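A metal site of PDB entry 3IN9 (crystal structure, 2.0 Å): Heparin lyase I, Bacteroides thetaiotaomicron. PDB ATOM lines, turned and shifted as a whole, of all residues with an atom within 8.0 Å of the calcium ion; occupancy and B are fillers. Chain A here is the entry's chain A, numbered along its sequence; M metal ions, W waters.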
ATOM      1  N   GLN A 123      35.178   5.272 -10.987  1.00  0.00           N
ATOM      2  CA  GLN A 123      33.918   5.790 -11.507  1.00  0.00           C
ATOM      3  C   GLN A 123      34.207   7.172 -12.089  1.00  0.00           C
ATOM      4  O   GLN A 123      35.044   7.915 -11.562  1.00  0.00           O
ATOM      5  CB  GLN A 123      32.916   5.964 -10.368  1.00  0.00           C
ATOM      6  CG  GLN A 123      32.072   4.753 -10.038  1.00  0.00           C
ATOM      7  CD  GLN A 123      31.048   4.498 -11.119  1.00  0.00           C
ATOM      8  OE1 GLN A 123      30.410   5.428 -11.610  1.00  0.00           O
ATOM      9  NE2 GLN A 123      30.882   3.223 -11.481  1.00  0.00           N
ATOM     10  N   MET A 153      31.623  -3.423 -12.034  1.00  0.00           N
ATOM     11  CA  MET A 153      31.966  -4.002 -10.743  1.00  0.00           C
ATOM     12  C   MET A 153      30.809  -3.624  -9.806  1.00  0.00           C
ATOM     13  O   MET A 153      30.849  -2.610  -9.119  1.00  0.00           O
ATOM     14  CB  MET A 153      33.294  -3.411 -10.243  1.00  0.00           C
ATOM     15  CG  MET A 153      34.471  -3.734 -11.149  1.00  0.00           C
ATOM     16  SD  MET A 153      36.006  -2.892 -10.712  1.00  0.00           S
ATOM     17  CE  MET A 153      36.570  -3.941  -9.364  1.00  0.00           C
ATOM     18  N   PRO A 154      29.747  -4.449  -9.797  1.00  0.00           N
ATOM     19  CA  PRO A 154      28.553  -4.207  -8.974  1.00  0.00           C
ATOM     20  C   PRO A 154      28.819  -3.995  -7.492  1.00  0.00           C
ATOM     21  O   PRO A 154      29.835  -4.435  -6.950  1.00  0.00           O
ATOM     22  CB  PRO A 154      27.712  -5.462  -9.223  1.00  0.00           C
ATOM     23  CG  PRO A 154      28.127  -5.894 -10.600  1.00  0.00           C
ATOM     24  CD  PRO A 154      29.612  -5.700 -10.568  1.00  0.00           C
ATOM     25  N   ASP A 155      27.882  -3.314  -6.835  1.00  0.00           N
ATOM     26  CA  ASP A 155      27.953  -3.065  -5.402  1.00  0.00           C
ATOM     27  C   ASP A 155      27.513  -4.374  -4.753  1.00  0.00           C
ATOM     28  O   ASP A 155      26.319  -4.626  -4.582  1.00  0.00           O
ATOM     29  CB  ASP A 155      27.024  -1.910  -5.044  1.00  0.00           C
ATOM     30  CG  ASP A 155      27.411  -0.606  -5.723  1.00  0.00           C
ATOM     31  OD1 ASP A 155      26.521   0.068  -6.307  1.00  0.00           O
ATOM     32  OD2 ASP A 155      28.610  -0.243  -5.686  1.00  0.00           O
ATOM     33  N   ARG A 156      28.493  -5.201  -4.398  1.00  0.00           N
ATOM     34  CA  ARG A 156      28.242  -6.518  -3.801  1.00  0.00           C
ATOM     35  C   ARG A 156      27.547  -6.551  -2.458  1.00  0.00           C
ATOM     36  O   ARG A 156      27.055  -7.598  -2.046  1.00  0.00           O
ATOM     37  CB  ARG A 156      29.568  -7.285  -3.679  1.00  0.00           C
ATOM     38  CG  ARG A 156      30.323  -7.426  -4.981  1.00  0.00           C
ATOM     39  CD  ARG A 156      29.624  -8.359  -5.946  1.00  0.00           C
ATOM     40  NE  ARG A 156      30.418  -8.538  -7.163  1.00  0.00           N
ATOM     41  CZ  ARG A 156      30.036  -9.274  -8.192  1.00  0.00           C
ATOM     42  NH1 ARG A 156      28.862  -9.907  -8.162  1.00  0.00           N
ATOM     43  NH2 ARG A 156      30.821  -9.385  -9.260  1.00  0.00           N
ATOM     44  N   LEU A 158      25.199  -4.099  -1.653  1.00  0.00           N
ATOM     45  CA  LEU A 158      23.998  -3.292  -1.808  1.00  0.00           C
ATOM     46  C   LEU A 158      22.827  -4.250  -1.980  1.00  0.00           C
ATOM     47  O   LEU A 158      22.794  -5.017  -2.934  1.00  0.00           O
ATOM     48  CB  LEU A 158      24.120  -2.396  -3.042  1.00  0.00           C
ATOM     49  CG  LEU A 158      22.943  -1.459  -3.318  1.00  0.00           C
ATOM     50  CD1 LEU A 158      22.783  -0.456  -2.162  1.00  0.00           C
ATOM     51  CD2 LEU A 158      23.189  -0.729  -4.645  1.00  0.00           C
ATOM     52  N   GLU A 222      22.871  -6.848  -5.568  1.00  0.00           N
ATOM     53  CA  GLU A 222      23.220  -6.447  -6.911  1.00  0.00           C
ATOM     54  C   GLU A 222      24.217  -7.417  -7.525  1.00  0.00           C
ATOM     55  O   GLU A 222      25.208  -7.784  -6.903  1.00  0.00           O
ATOM     56  CB  GLU A 222      23.785  -5.044  -6.944  1.00  0.00           C
ATOM     57  CG  GLU A 222      24.036  -4.607  -8.358  1.00  0.00           C
ATOM     58  CD  GLU A 222      24.325  -3.146  -8.467  1.00  0.00           C
ATOM     59  OE1 GLU A 222      25.425  -2.735  -8.052  1.00  0.00           O
ATOM     60  OE2 GLU A 222      23.450  -2.419  -8.954  1.00  0.00           O
ATOM     61  N   GLN A 223      23.944  -7.834  -8.757  1.00  0.00           N
ATOM     62  CA  GLN A 223      24.784  -8.792  -9.451  1.00  0.00           C
ATOM     63  C   GLN A 223      24.462  -8.705 -10.936  1.00  0.00           C
ATOM     64  O   GLN A 223      23.360  -8.308 -11.299  1.00  0.00           O
ATOM     65  CB  GLN A 223      24.485 -10.200  -8.911  1.00  0.00           C
ATOM     66  CG  GLN A 223      25.250 -11.352  -9.542  1.00  0.00           C
ATOM     67  CD  GLN A 223      24.729 -11.706 -10.922  1.00  0.00           C
ATOM     68  OE1 GLN A 223      23.522 -11.691 -11.171  1.00  0.00           O
ATOM     69  NE2 GLN A 223      25.629 -12.060 -11.834  1.00  0.00           N
ATOM     70  N   ASP A 245      23.524   2.312 -16.951  1.00  0.00           N
ATOM     71  CA  ASP A 245      22.542   1.897 -15.959  1.00  0.00           C
ATOM     72  C   ASP A 245      22.657   2.866 -14.789  1.00  0.00           C
ATOM     73  O   ASP A 245      23.576   2.753 -13.977  1.00  0.00           O
ATOM     74  CB  ASP A 245      22.849   0.473 -15.499  1.00  0.00           C
ATOM     75  CG  ASP A 245      21.746  -0.122 -14.638  1.00  0.00           C
ATOM     76  OD1 ASP A 245      20.862   0.629 -14.197  1.00  0.00           O
ATOM     77  OD2 ASP A 245      21.782  -1.341 -14.391  1.00  0.00           O
ATOM     78  N   ARG A 246      21.716   3.804 -14.702  1.00  0.00           N
ATOM     79  CA  ARG A 246      21.781   4.787 -13.630  1.00  0.00           C
ATOM     80  C   ARG A 246      21.040   4.374 -12.370  1.00  0.00           C
ATOM     81  O   ARG A 246      21.043   5.103 -11.375  1.00  0.00           O
ATOM     82  CB  ARG A 246      21.263   6.160 -14.114  1.00  0.00           C
ATOM     83  CG  ARG A 246      19.757   6.259 -14.234  1.00  0.00           C
ATOM     84  CD  ARG A 246      19.343   7.603 -14.851  1.00  0.00           C
ATOM     85  NE  ARG A 246      17.934   7.576 -15.229  1.00  0.00           N
ATOM     86  CZ  ARG A 246      16.943   8.019 -14.461  1.00  0.00           C
ATOM     87  NH1 ARG A 246      17.190   8.537 -13.265  1.00  0.00           N
ATOM     88  NH2 ARG A 246      15.691   7.905 -14.889  1.00  0.00           N
ATOM     89  N   LYS A 247      20.402   3.206 -12.376  1.00  0.00           N
ATOM     90  CA  LYS A 247      19.685   2.770 -11.191  1.00  0.00           C
ATOM     91  C   LYS A 247      20.732   2.445 -10.133  1.00  0.00           C
ATOM     92  O   LYS A 247      21.789   1.889 -10.445  1.00  0.00           O
ATOM     93  CB  LYS A 247      18.793   1.555 -11.469  1.00  0.00           C
ATOM     94  CG  LYS A 247      17.751   1.317 -10.388  1.00  0.00           C
ATOM     95  CD  LYS A 247      16.802   0.166 -10.743  1.00  0.00           C
ATOM     96  CE  LYS A 247      15.676   0.032  -9.720  1.00  0.00           C
ATOM     97  NZ  LYS A 247      16.164  -0.384  -8.378  1.00  0.00           N
ATOM     98  N   TRP A 248      20.450   2.802  -8.884  1.00  0.00           N
ATOM     99  CA  TRP A 248      21.385   2.563  -7.781  1.00  0.00           C
ATOM    100  C   TRP A 248      21.564   1.047  -7.610  1.00  0.00           C
ATOM    101  O   TRP A 248      22.685   0.567  -7.522  1.00  0.00           O
ATOM    102  CB  TRP A 248      20.868   3.223  -6.501  1.00  0.00           C
ATOM    103  CG  TRP A 248      21.772   3.145  -5.290  1.00  0.00           C
ATOM    104  CD1 TRP A 248      21.388   2.965  -3.994  1.00  0.00           C
ATOM    105  CD2 TRP A 248      23.195   3.284  -5.267  1.00  0.00           C
ATOM    106  NE1 TRP A 248      22.485   2.976  -3.164  1.00  0.00           N
ATOM    107  CE2 TRP A 248      23.611   3.166  -3.919  1.00  0.00           C
ATOM    108  CE3 TRP A 248      24.172   3.497  -6.260  1.00  0.00           C
ATOM    109  CZ2 TRP A 248      24.948   3.255  -3.526  1.00  0.00           C
ATOM    110  CZ3 TRP A 248      25.508   3.586  -5.867  1.00  0.00           C
ATOM    111  CH2 TRP A 248      25.878   3.461  -4.507  1.00  0.00           C
ATOM    112  N   LEU A 249      20.455   0.310  -7.553  1.00  0.00           N
ATOM    113  CA  LEU A 249      20.501  -1.153  -7.430  1.00  0.00           C
ATOM    114  C   LEU A 249      19.988  -1.689  -8.773  1.00  0.00           C
ATOM    115  O   LEU A 249      18.782  -1.683  -9.045  1.00  0.00           O
ATOM    116  CB  LEU A 249      19.588  -1.647  -6.301  1.00  0.00           C
ATOM    117  CG  LEU A 249      19.960  -2.971  -5.617  1.00  0.00           C
ATOM    118  CD1 LEU A 249      18.822  -3.404  -4.719  1.00  0.00           C
ATOM    119  CD2 LEU A 249      20.255  -4.063  -6.633  1.00  0.00           C
ATOM    120  N   THR A 250      20.902  -2.136  -9.617  1.00  0.00           N
ATOM    121  CA  THR A 250      20.548  -2.638 -10.934  1.00  0.00           C
ATOM    122  C   THR A 250      19.379  -3.604 -10.945  1.00  0.00           C
ATOM    123  O   THR A 250      19.270  -4.492 -10.096  1.00  0.00           O
ATOM    124  CB  THR A 250      21.769  -3.310 -11.620  1.00  0.00           C
ATOM    125  OG1 THR A 250      22.708  -2.297 -12.009  1.00  0.00           O
ATOM    126  CG2 THR A 250      21.332  -4.071 -12.854  1.00  0.00           C
ATOM    127  N   ASP A 251      18.493  -3.434 -11.921  1.00  0.00           N
ATOM    128  CA  ASP A 251      17.318  -4.269 -12.088  1.00  0.00           C
ATOM    129  C   ASP A 251      17.583  -5.192 -13.270  1.00  0.00           C
ATOM    130  O   ASP A 251      17.531  -4.756 -14.426  1.00  0.00           O
ATOM    131  CB  ASP A 251      16.085  -3.398 -12.356  1.00  0.00           C
ATOM    132  CG  ASP A 251      14.848  -4.205 -12.679  1.00  0.00           C
ATOM    133  OD1 ASP A 251      14.887  -5.454 -12.560  1.00  0.00           O
ATOM    134  OD2 ASP A 251      13.830  -3.594 -13.055  1.00  0.00           O
ATOM    135  N   LYS A 306      24.714   8.231  -7.518  1.00  0.00           N
ATOM    136  CA  LYS A 306      24.538   7.271  -6.442  1.00  0.00           C
ATOM    137  C   LYS A 306      23.064   7.081  -6.073  1.00  0.00           C
ATOM    138  O   LYS A 306      22.237   6.780  -6.944  1.00  0.00           O
ATOM    139  CB  LYS A 306      25.310   7.749  -5.199  1.00  0.00           C
ATOM    140  CG  LYS A 306      26.792   8.006  -5.458  1.00  0.00           C
ATOM    141  CD  LYS A 306      27.588   6.719  -5.564  1.00  0.00           C
ATOM    142  CE  LYS A 306      29.054   6.998  -5.876  1.00  0.00           C
ATOM    143  NZ  LYS A 306      29.635   7.984  -4.914  1.00  0.00           N
ATOM    144  N   ARG A 344      27.877   2.393 -15.155  1.00  0.00           N
ATOM    145  CA  ARG A 344      26.914   1.885 -14.192  1.00  0.00           C
ATOM    146  C   ARG A 344      27.005   2.735 -12.933  1.00  0.00           C
ATOM    147  O   ARG A 344      28.085   3.196 -12.572  1.00  0.00           O
ATOM    148  CB  ARG A 344      27.250   0.438 -13.820  1.00  0.00           C
ATOM    149  CG  ARG A 344      27.101  -0.604 -14.926  1.00  0.00           C
ATOM    150  CD  ARG A 344      27.725  -1.918 -14.460  1.00  0.00           C
ATOM    151  NE  ARG A 344      27.289  -2.232 -13.108  1.00  0.00           N
ATOM    152  CZ  ARG A 344      26.112  -2.752 -12.798  1.00  0.00           C
ATOM    153  NH1 ARG A 344      25.240  -3.051 -13.748  1.00  0.00           N
ATOM    154  NH2 ARG A 344      25.785  -2.953 -11.524  1.00  0.00           N
ATOM    155  N   ASN A 345      25.871   2.937 -12.291  1.00  0.00           N
ATOM    156  CA  ASN A 345      25.813   3.724 -11.069  1.00  0.00           C
ATOM    157  C   ASN A 345      26.308   2.821  -9.918  1.00  0.00           C
ATOM    158  O   ASN A 345      25.501   2.348  -9.113  1.00  0.00           O
ATOM    159  CB  ASN A 345      24.380   4.200 -10.819  1.00  0.00           C
ATOM    160  CG  ASN A 345      24.258   5.022  -9.562  1.00  0.00           C
ATOM    161  OD1 ASN A 345      25.268   5.348  -8.938  1.00  0.00           O
ATOM    162  ND2 ASN A 345      23.025   5.382  -9.184  1.00  0.00           N
ATOM    163  N   ASP A 346      27.619   2.577  -9.869  1.00  0.00           N
ATOM    164  CA  ASP A 346      28.237   1.743  -8.837  1.00  0.00           C
ATOM    165  C   ASP A 346      29.250   2.556  -8.047  1.00  0.00           C
ATOM    166  O   ASP A 346      29.576   3.696  -8.391  1.00  0.00           O
ATOM    167  CB  ASP A 346      29.036   0.563  -9.431  1.00  0.00           C
ATOM    168  CG  ASP A 346      28.180  -0.436 -10.169  1.00  0.00           C
ATOM    169  OD1 ASP A 346      26.976  -0.510  -9.897  1.00  0.00           O
ATOM    170  OD2 ASP A 346      28.724  -1.180 -11.017  1.00  0.00           O
ATOM    171  N   GLU A 347      29.776   1.953  -6.979  1.00  0.00           N
ATOM    172  CA  GLU A 347      30.804   2.584  -6.166  1.00  0.00           C
ATOM    173  C   GLU A 347      32.110   2.407  -6.945  1.00  0.00           C
ATOM    174  O   GLU A 347      32.868   3.354  -7.155  1.00  0.00           O
ATOM    175  CB  GLU A 347      30.918   1.871  -4.815  1.00  0.00           C
ATOM    176  CG  GLU A 347      31.990   2.452  -3.900  1.00  0.00           C
ATOM    177  CD  GLU A 347      32.203   1.611  -2.651  1.00  0.00           C
ATOM    178  OE1 GLU A 347      31.202   1.065  -2.116  1.00  0.00           O
ATOM    179  OE2 GLU A 347      33.355   1.502  -2.194  1.00  0.00           O
ATOM    180  N   ASP A 348      32.340   1.168  -7.382  1.00  0.00           N
ATOM    181  CA  ASP A 348      33.540   0.817  -8.141  1.00  0.00           C
ATOM    182  C   ASP A 348      33.408   1.071  -9.633  1.00  0.00           C
ATOM    183  O   ASP A 348      32.308   1.211 -10.176  1.00  0.00           O
ATOM    184  CB  ASP A 348      33.914  -0.649  -7.906  1.00  0.00           C
ATOM    185  CG  ASP A 348      34.684  -0.858  -6.626  1.00  0.00           C
ATOM    186  OD1 ASP A 348      34.754   0.083  -5.819  1.00  0.00           O
ATOM    187  OD2 ASP A 348      35.212  -1.964  -6.430  1.00  0.00           O
HETATM  188 CA    CA M   1      24.887  -0.160  -8.570  1.00  0.00          CA
HETATM  189  O   HOH W   1      23.738   0.143 -10.930  1.00  0.00           O
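Water W1 bridges the backbone carbonyl oxygen (O) of Lys 247 and the side-chain hydroxyl (OG1) of Thr 250.
OD2 of Asp 155 is in hydrogen-bond range of N of Glu 347, at 2.8 Å. The backbone carbonyl oxygen (O) of Leu 158 sits at hydrogen-bond distance from the backbone NH (N) of Glu 222 (3.2 Å). The side-chain amide nitrogen (ND2) of Asn 345 lies within hydrogen-bond range of the backbone carbonyl oxygen (O) of Arg 246 (3.0 Å). O of Asp 245 sits at hydrogen-bond distance from N of Asn 345, 2.9 Å away. The guanidinium group (NE) of Arg 344 is in salt-bridge range of the side-chain carboxylate (OD2) of Asp 346 (2.7 Å). NE2 of Gln 123 lies close to O of Asp 346 (3.4 Å). The backbone NH (N) of Thr 250 sits close to the side-chain carboxylate (OE2) of Glu 222, at 2.6 Å. ND2 of Asn 345 sits at hydrogen-bond distance from O of Lys 306 (2.8 Å).
The calcium ion is bound by OD1 of Asp 346 (2.5 Å). The calcium ion is bound by the backbone carbonyl oxygen (O) of Trp 248 (2.5 Å). The backbone carbonyl oxygen (O) of Asn 345 binds the calcium ion (2.6 Å). The calcium ion is bound by water W1 (2.6 Å). The calcium ion is bound by OE1 of Glu 222 (2.7 Å). OE2 of Glu 222 is bound to the calcium ion (2.7 Å). OD1 of Asp 155 binds the calcium ion, at 2.8 Å.
The nearest printed residue that does not touch the calcium ion is Lys 247 (4.2 Å).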
